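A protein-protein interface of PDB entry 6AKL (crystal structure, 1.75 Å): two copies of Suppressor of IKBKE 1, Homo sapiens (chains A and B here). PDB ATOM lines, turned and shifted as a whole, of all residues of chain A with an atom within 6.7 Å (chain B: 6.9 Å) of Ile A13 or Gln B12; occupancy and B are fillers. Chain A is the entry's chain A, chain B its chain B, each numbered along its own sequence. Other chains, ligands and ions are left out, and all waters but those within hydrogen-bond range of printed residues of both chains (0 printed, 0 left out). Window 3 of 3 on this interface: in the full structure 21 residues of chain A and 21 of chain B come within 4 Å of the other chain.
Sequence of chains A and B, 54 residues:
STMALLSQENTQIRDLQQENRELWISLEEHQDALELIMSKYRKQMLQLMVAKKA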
ATOM      1  N   GLN A   8       7.652  -6.064   9.242  1.00  0.00           N
ATOM      2  CA  GLN A   8       6.653  -5.138   9.767  1.00  0.00           C
ATOM      3  C   GLN A   8       6.911  -4.808  11.232  1.00  0.00           C
ATOM      4  O   GLN A   8       6.801  -3.646  11.645  1.00  0.00           O
ATOM      5  CB  GLN A   8       5.252  -5.725   9.591  1.00  0.00           C
ATOM      6  N   GLU A   9       7.244  -5.818  12.039  1.00  0.00           N
ATOM      7  CA  GLU A   9       7.504  -5.564  13.451  1.00  0.00           C
ATOM      8  C   GLU A   9       8.766  -4.729  13.631  1.00  0.00           C
ATOM      9  O   GLU A   9       8.792  -3.806  14.457  1.00  0.00           O
ATOM     10  CB  GLU A   9       7.588  -6.890  14.219  1.00  0.00           C
ATOM     11  CG  GLU A   9       8.931  -7.628  14.158  1.00  0.00           C
ATOM     12  CD  GLU A   9       9.068  -8.563  12.957  1.00  0.00           C
ATOM     13  OE1 GLU A   9      10.150  -9.174  12.800  1.00  0.00           O
ATOM     14  OE2 GLU A   9       8.105  -8.687  12.169  1.00  0.00           O
ATOM     15  N   ASN A  10       9.809  -5.004  12.842  1.00  0.00           N
ATOM     16  CA  ASN A  10      11.065  -4.291  13.036  1.00  0.00           C
ATOM     17  C   ASN A  10      10.981  -2.853  12.555  1.00  0.00           C
ATOM     18  O   ASN A  10      11.609  -1.978  13.155  1.00  0.00           O
ATOM     19  CB  ASN A  10      12.212  -5.008  12.336  1.00  0.00           C
ATOM     20  CG  ASN A  10      12.620  -6.267  13.059  1.00  0.00           C
ATOM     21  OD1 ASN A  10      12.291  -6.448  14.235  1.00  0.00           O
ATOM     22  ND2 ASN A  10      13.348  -7.145  12.368  1.00  0.00           N
ATOM     23  N   THR A  11      10.225  -2.583  11.483  1.00  0.00           N
ATOM     24  CA  THR A  11      10.048  -1.192  11.079  1.00  0.00           C
ATOM     25  C   THR A  11       9.215  -0.422  12.095  1.00  0.00           C
ATOM     26  O   THR A  11       9.457   0.769  12.293  1.00  0.00           O
ATOM     27  CB  THR A  11       9.403  -1.079   9.692  1.00  0.00           C
ATOM     28  OG1 THR A  11       8.067  -1.591   9.729  1.00  0.00           O
ATOM     29  CG2 THR A  11      10.209  -1.829   8.651  1.00  0.00           C
ATOM     30  N   GLN A  12       8.220  -1.064  12.728  1.00  0.00           N
ATOM     31  CA  GLN A  12       7.484  -0.384  13.801  1.00  0.00           C
ATOM     32  C   GLN A  12       8.420  -0.003  14.936  1.00  0.00           C
ATOM     33  O   GLN A  12       8.369   1.119  15.463  1.00  0.00           O
ATOM     34  CB  GLN A  12       6.368  -1.285  14.337  1.00  0.00           C
ATOM     35  CG  GLN A  12       5.103  -1.329  13.526  1.00  0.00           C
ATOM     36  CD  GLN A  12       4.010  -2.110  14.247  1.00  0.00           C
ATOM     37  OE1 GLN A  12       3.605  -1.754  15.355  1.00  0.00           O
ATOM     38  NE2 GLN A  12       3.546  -3.186  13.628  1.00  0.00           N
ATOM     39  N   ILE A  13       9.259  -0.952  15.353  1.00  0.00           N
ATOM     40  CA  ILE A  13      10.240  -0.692  16.401  1.00  0.00           C
ATOM     41  C   ILE A  13      11.191   0.421  15.977  1.00  0.00           C
ATOM     42  O   ILE A  13      11.441   1.361  16.739  1.00  0.00           O
ATOM     43  CB  ILE A  13      10.996  -1.990  16.742  1.00  0.00           C
ATOM     44  CG1 ILE A  13      10.074  -2.942  17.505  1.00  0.00           C
ATOM     45  CG2 ILE A  13      12.281  -1.681  17.515  1.00  0.00           C
ATOM     46  CD1 ILE A  13      10.696  -4.340  17.739  1.00  0.00           C
ATOM     47  N   ARG A  14      11.751   0.312  14.762  1.00  0.00           N
ATOM     48  CA  ARG A  14      12.711   1.284  14.255  1.00  0.00           C
ATOM     49  C   ARG A  14      12.098   2.679  14.161  1.00  0.00           C
ATOM     50  O   ARG A  14      12.750   3.671  14.508  1.00  0.00           O
ATOM     51  CB  ARG A  14      13.234   0.842  12.878  1.00  0.00           C
ATOM     52  CG  ARG A  14      14.425  -0.121  12.904  1.00  0.00           C
ATOM     53  CD  ARG A  14      14.768  -0.683  11.483  1.00  0.00           C
ATOM     54  NE  ARG A  14      15.370   0.321  10.590  1.00  0.00           N
ATOM     55  CZ  ARG A  14      16.645   0.708  10.653  1.00  0.00           C
ATOM     56  NH1 ARG A  14      17.441   0.195  11.584  1.00  0.00           N
ATOM     57  NH2 ARG A  14      17.132   1.604   9.795  1.00  0.00           N
ATOM     58  N   ASP A  15      10.845   2.777  13.697  1.00  0.00           N
ATOM     59  CA  ASP A  15      10.189   4.083  13.617  1.00  0.00           C
ATOM     60  C   ASP A  15       9.997   4.699  14.996  1.00  0.00           C
ATOM     61  O   ASP A  15      10.149   5.919  15.165  1.00  0.00           O
ATOM     62  CB  ASP A  15       8.834   3.972  12.917  1.00  0.00           C
ATOM     63  CG  ASP A  15       8.966   3.853  11.405  1.00  0.00           C
ATOM     64  OD1 ASP A  15      10.081   4.055  10.887  1.00  0.00           O
ATOM     65  OD2 ASP A  15       7.946   3.565  10.747  1.00  0.00           O
ATOM     66  N   LEU A  16       9.621   3.875  15.983  1.00  0.00           N
ATOM     67  CA  LEU A  16       9.461   4.395  17.335  1.00  0.00           C
ATOM     68  C   LEU A  16      10.810   4.801  17.917  1.00  0.00           C
ATOM     69  O   LEU A  16      10.928   5.838  18.572  1.00  0.00           O
ATOM     70  CB  LEU A  16       8.776   3.346  18.216  1.00  0.00           C
ATOM     71  CG  LEU A  16       7.250   3.288  18.117  1.00  0.00           C
ATOM     72  CD1 LEU A  16       6.715   1.908  18.541  1.00  0.00           C
ATOM     73  CD2 LEU A  16       6.620   4.396  18.971  1.00  0.00           C
ATOM     74  N   GLN A  17      11.848   4.000  17.683  1.00  0.00           N
ATOM     75  CA  GLN A  17      13.167   4.389  18.170  1.00  0.00           C
ATOM     76  C   GLN A  17      13.624   5.697  17.525  1.00  0.00           C
ATOM     77  O   GLN A  17      14.213   6.547  18.197  1.00  0.00           O
ATOM     78  CB  GLN A  17      14.171   3.264  17.901  1.00  0.00           C
ATOM     79  CG  GLN A  17      13.866   2.024  18.713  1.00  0.00           C
ATOM     80  CD  GLN A  17      14.830   0.879  18.425  1.00  0.00           C
ATOM     81  OE1 GLN A  17      15.203   0.127  19.335  1.00  0.00           O
ATOM     82  NE2 GLN A  17      15.235   0.746  17.172  1.00  0.00           N
ATOM     83  N   GLN A  18      13.385   5.860  16.218  1.00  0.00           N
ATOM     84  CA  GLN A  18      13.793   7.090  15.535  1.00  0.00           C
ATOM     85  C   GLN A  18      13.041   8.307  16.081  1.00  0.00           C
ATOM     86  O   GLN A  18      13.639   9.365  16.296  1.00  0.00           O
ATOM     87  CB  GLN A  18      13.587   6.965  14.013  1.00  0.00           C
ATOM     88  CG  GLN A  18      13.678   8.338  13.228  1.00  0.00           C
ATOM     89  CD  GLN A  18      13.300   8.234  11.734  1.00  0.00           C
ATOM     90  OE1 GLN A  18      12.672   7.269  11.289  1.00  0.00           O
ATOM     91  NE2 GLN A  18      13.684   9.246  10.963  1.00  0.00           N
ATOM     92  N   SER B   7       4.171 -11.624  21.977  1.00  0.00           N
ATOM     93  CA  SER B   7       5.601 -11.889  21.919  1.00  0.00           C
ATOM     94  C   SER B   7       6.391 -10.748  22.556  1.00  0.00           C
ATOM     95  O   SER B   7       5.832  -9.758  23.035  1.00  0.00           O
ATOM     96  CB  SER B   7       6.040 -12.093  20.472  1.00  0.00           C
ATOM     97  OG  SER B   7       5.921 -10.880  19.748  1.00  0.00           O
ATOM     98  N   GLN B   8       7.722 -10.873  22.539  1.00  0.00           N
ATOM     99  CA  GLN B   8       8.560  -9.841  23.142  1.00  0.00           C
ATOM    100  C   GLN B   8       8.738  -8.638  22.221  1.00  0.00           C
ATOM    101  O   GLN B   8       8.987  -7.527  22.704  1.00  0.00           O
ATOM    102  CB  GLN B   8       9.919 -10.425  23.542  1.00  0.00           C
ATOM    103  CG  GLN B   8      10.942 -10.520  22.422  1.00  0.00           C
ATOM    104  CD  GLN B   8      12.357 -10.693  22.949  1.00  0.00           C
ATOM    105  OE1 GLN B   8      12.596 -10.612  24.155  1.00  0.00           O
ATOM    106  NE2 GLN B   8      13.300 -10.942  22.046  1.00  0.00           N
ATOM    107  N   GLU B   9       8.611  -8.826  20.906  1.00  0.00           N
ATOM    108  CA  GLU B   9       8.592  -7.677  20.007  1.00  0.00           C
ATOM    109  C   GLU B   9       7.371  -6.810  20.276  1.00  0.00           C
ATOM    110  O   GLU B   9       7.451  -5.574  20.229  1.00  0.00           O
ATOM    111  CB  GLU B   9       8.616  -8.140  18.547  1.00  0.00           C
ATOM    112  CG  GLU B   9       9.918  -8.810  18.115  1.00  0.00           C
ATOM    113  CD  GLU B   9      10.081 -10.215  18.693  1.00  0.00           C
ATOM    114  OE1 GLU B   9       9.053 -10.862  18.999  1.00  0.00           O
ATOM    115  OE2 GLU B   9      11.235 -10.670  18.844  1.00  0.00           O
ATOM    116  N   ASN B  10       6.229  -7.438  20.563  1.00  0.00           N
ATOM    117  CA  ASN B  10       5.052  -6.668  20.952  1.00  0.00           C
ATOM    118  C   ASN B  10       5.266  -5.962  22.280  1.00  0.00           C
ATOM    119  O   ASN B  10       4.785  -4.838  22.467  1.00  0.00           O
ATOM    120  CB  ASN B  10       3.825  -7.570  21.024  1.00  0.00           C
ATOM    121  CG  ASN B  10       3.327  -7.974  19.656  1.00  0.00           C
ATOM    122  OD1 ASN B  10       3.960  -7.665  18.642  1.00  0.00           O
ATOM    123  ND2 ASN B  10       2.199  -8.676  19.614  1.00  0.00           N
ATOM    124  N   THR B  11       5.987  -6.595  23.209  1.00  0.00           N
ATOM    125  CA  THR B  11       6.306  -5.924  24.461  1.00  0.00           C
ATOM    126  C   THR B  11       7.233  -4.739  24.219  1.00  0.00           C
ATOM    127  O   THR B  11       7.031  -3.664  24.799  1.00  0.00           O
ATOM    128  CB  THR B  11       6.925  -6.912  25.448  1.00  0.00           C
ATOM    129  OG1 THR B  11       5.953  -7.915  25.774  1.00  0.00           O
ATOM    130  CG2 THR B  11       7.352  -6.191  26.729  1.00  0.00           C
ATOM    131  N   GLN B  12       8.230  -4.907  23.343  1.00  0.00           N
ATOM    132  CA  GLN B  12       9.154  -3.812  23.049  1.00  0.00           C
ATOM    133  C   GLN B  12       8.433  -2.658  22.363  1.00  0.00           C
ATOM    134  O   GLN B  12       8.719  -1.488  22.635  1.00  0.00           O
ATOM    135  CB  GLN B  12      10.314  -4.313  22.181  1.00  0.00           C
ATOM    136  CG  GLN B  12      11.456  -3.314  22.044  1.00  0.00           C
ATOM    137  CD  GLN B  12      12.569  -3.796  21.114  1.00  0.00           C
ATOM    138  OE1 GLN B  12      12.474  -4.867  20.510  1.00  0.00           O
ATOM    139  NE2 GLN B  12      13.631  -3.001  20.999  1.00  0.00           N
ATOM    140  N   ILE B  13       7.470  -2.965  21.494  1.00  0.00           N
ATOM    141  CA  ILE B  13       6.680  -1.909  20.865  1.00  0.00           C
ATOM    142  C   ILE B  13       5.864  -1.156  21.908  1.00  0.00           C
ATOM    143  O   ILE B  13       5.821   0.080  21.912  1.00  0.00           O
ATOM    144  CB  ILE B  13       5.783  -2.492  19.758  1.00  0.00           C
ATOM    145  CG1 ILE B  13       6.633  -2.961  18.581  1.00  0.00           C
ATOM    146  CG2 ILE B  13       4.756  -1.440  19.303  1.00  0.00           C
ATOM    147  CD1 ILE B  13       5.883  -3.805  17.565  1.00  0.00           C
ATOM    148  N   ARG B  14       5.202  -1.886  22.814  1.00  0.00           N
ATOM    149  CA  ARG B  14       4.377  -1.222  23.821  1.00  0.00           C
ATOM    150  C   ARG B  14       5.225  -0.353  24.736  1.00  0.00           C
ATOM    151  O   ARG B  14       4.809   0.750  25.114  1.00  0.00           O
ATOM    152  CB  ARG B  14       3.589  -2.256  24.637  1.00  0.00           C
ATOM    153  CG  ARG B  14       2.217  -2.579  24.041  1.00  0.00           C
ATOM    154  CD  ARG B  14       1.452  -3.633  24.837  1.00  0.00           C
ATOM    155  NE  ARG B  14       1.345  -4.904  24.120  1.00  0.00           N
ATOM    156  CZ  ARG B  14       0.351  -5.236  23.296  1.00  0.00           C
ATOM    157  NH1 ARG B  14      -0.650  -4.397  23.073  1.00  0.00           N
ATOM    158  NH2 ARG B  14       0.357  -6.419  22.698  1.00  0.00           N
ATOM    159  N   ASP B  15       6.425  -0.826  25.093  1.00  0.00           N
ATOM    160  CA  ASP B  15       7.331  -0.024  25.921  1.00  0.00           C
ATOM    161  C   ASP B  15       7.783   1.239  25.193  1.00  0.00           C
ATOM    162  O   ASP B  15       7.892   2.314  25.799  1.00  0.00           O
ATOM    163  CB  ASP B  15       8.557  -0.849  26.317  1.00  0.00           C
ATOM    164  CG  ASP B  15       8.243  -1.889  27.390  1.00  0.00           C
ATOM    165  OD1 ASP B  15       7.137  -1.835  27.978  1.00  0.00           O
ATOM    166  OD2 ASP B  15       9.103  -2.764  27.636  1.00  0.00           O
ATOM    167  N   LEU B  16       8.069   1.117  23.893  1.00  0.00           N
ATOM    168  CA  LEU B  16       8.507   2.271  23.118  1.00  0.00           C
ATOM    169  C   LEU B  16       7.374   3.263  22.926  1.00  0.00           C
ATOM    170  O   LEU B  16       7.617   4.477  22.878  1.00  0.00           O
ATOM    171  CB  LEU B  16       9.041   1.820  21.752  1.00  0.00           C
ATOM    172  CG  LEU B  16      10.437   1.182  21.736  1.00  0.00           C
ATOM    173  CD1 LEU B  16      10.717   0.433  20.406  1.00  0.00           C
ATOM    174  CD2 LEU B  16      11.477   2.233  21.961  1.00  0.00           C
ATOM    175  N   GLN B  17       6.136   2.778  22.794  1.00  0.00           N
ATOM    176  CA  GLN B  17       5.015   3.709  22.667  1.00  0.00           C
ATOM    177  C   GLN B  17       4.784   4.469  23.963  1.00  0.00           C
ATOM    178  O   GLN B  17       4.528   5.676  23.943  1.00  0.00           O
ATOM    179  CB  GLN B  17       3.754   2.956  22.242  1.00  0.00           C
ATOM    180  CG  GLN B  17       3.905   2.332  20.863  1.00  0.00           C
ATOM    181  CD  GLN B  17       2.761   1.396  20.494  1.00  0.00           C
ATOM    182  OE1 GLN B  17       2.406   1.263  19.321  1.00  0.00           O
ATOM    183  NE2 GLN B  17       2.203   0.729  21.485  1.00  0.00           N
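Hydrophobic or aromatic side chains of chain A within 4 Å of the printed part of chain B: Ile A13 and Leu A16.
Gln A12 touches Ile B13, and with the chains exchanged Ile A13 touches Gln B12.
Ile A13 touches Leu B16, and with the chains exchanged Leu A16 touches Ile B13.
Leu A16 touches Gln B17, and with the chains exchanged Gln A17 touches Leu B16.
Gln A17 touches Gln B12, but with the chains exchanged Gln A12 does not touch Gln B17 (5.1 Å).
10 positions are printed for both chains.
Of the 9 pairs that touch across the chains among the printed residues, 8 have their exchanged pair printed and touching as well.
Among the printed residues, merely in contact across the chains: Gln A12 with Ile B13 (3.8 Å), Ile A13 with Gln B12 (3.3 Å), Ile A13 with Ile B13 (3.6 Å), Ile A13 with Leu B16 (3.9 Å), Leu A16 with Ile B13 (3.9 Å), Leu A16 with Leu B16 (3.9 Å), Leu A16 with Gln B17 (3.7 Å), Gln A17 with Gln B12 (3.9 Å) and Gln A17 with Leu B16 (3.9 Å).
Of chain B, only Gln B12 (3.3 Å), Ile B13 (3.6 Å) and Leu B16 (3.9 Å) come within 4 Å of Ile A13.
Gln B12 touches two residues of chain A.
Of the printed residues of chain B, Leu A16 touches Ile B13 (3.9 Å), Leu B16 (3.9 Å) and Gln B17 (3.7 Å).
Printed residues of chain A within 4 Å of Gln B17: Leu A16 (3.7 Å).
Printed residues of chain B within 4 Å of Gln A12: Ile B13.
Of the printed residues of chain B, Gln A17 touches Gln B12 and Leu B16.
Printed residues of chain A within 4 Å of Leu B16: Ile A13 (3.9 Å), Leu A16 (3.9 Å) and Gln A17 (3.9 Å).
Arg A14 touches none of the printed residues of chain B.
The nearest residue of chain B that does not touch Ile A13 is Glu B9 (4.3 Å).
The nearest printed residue of chain A that does not touch Ile B13 is Glu A9 (4.3 Å).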
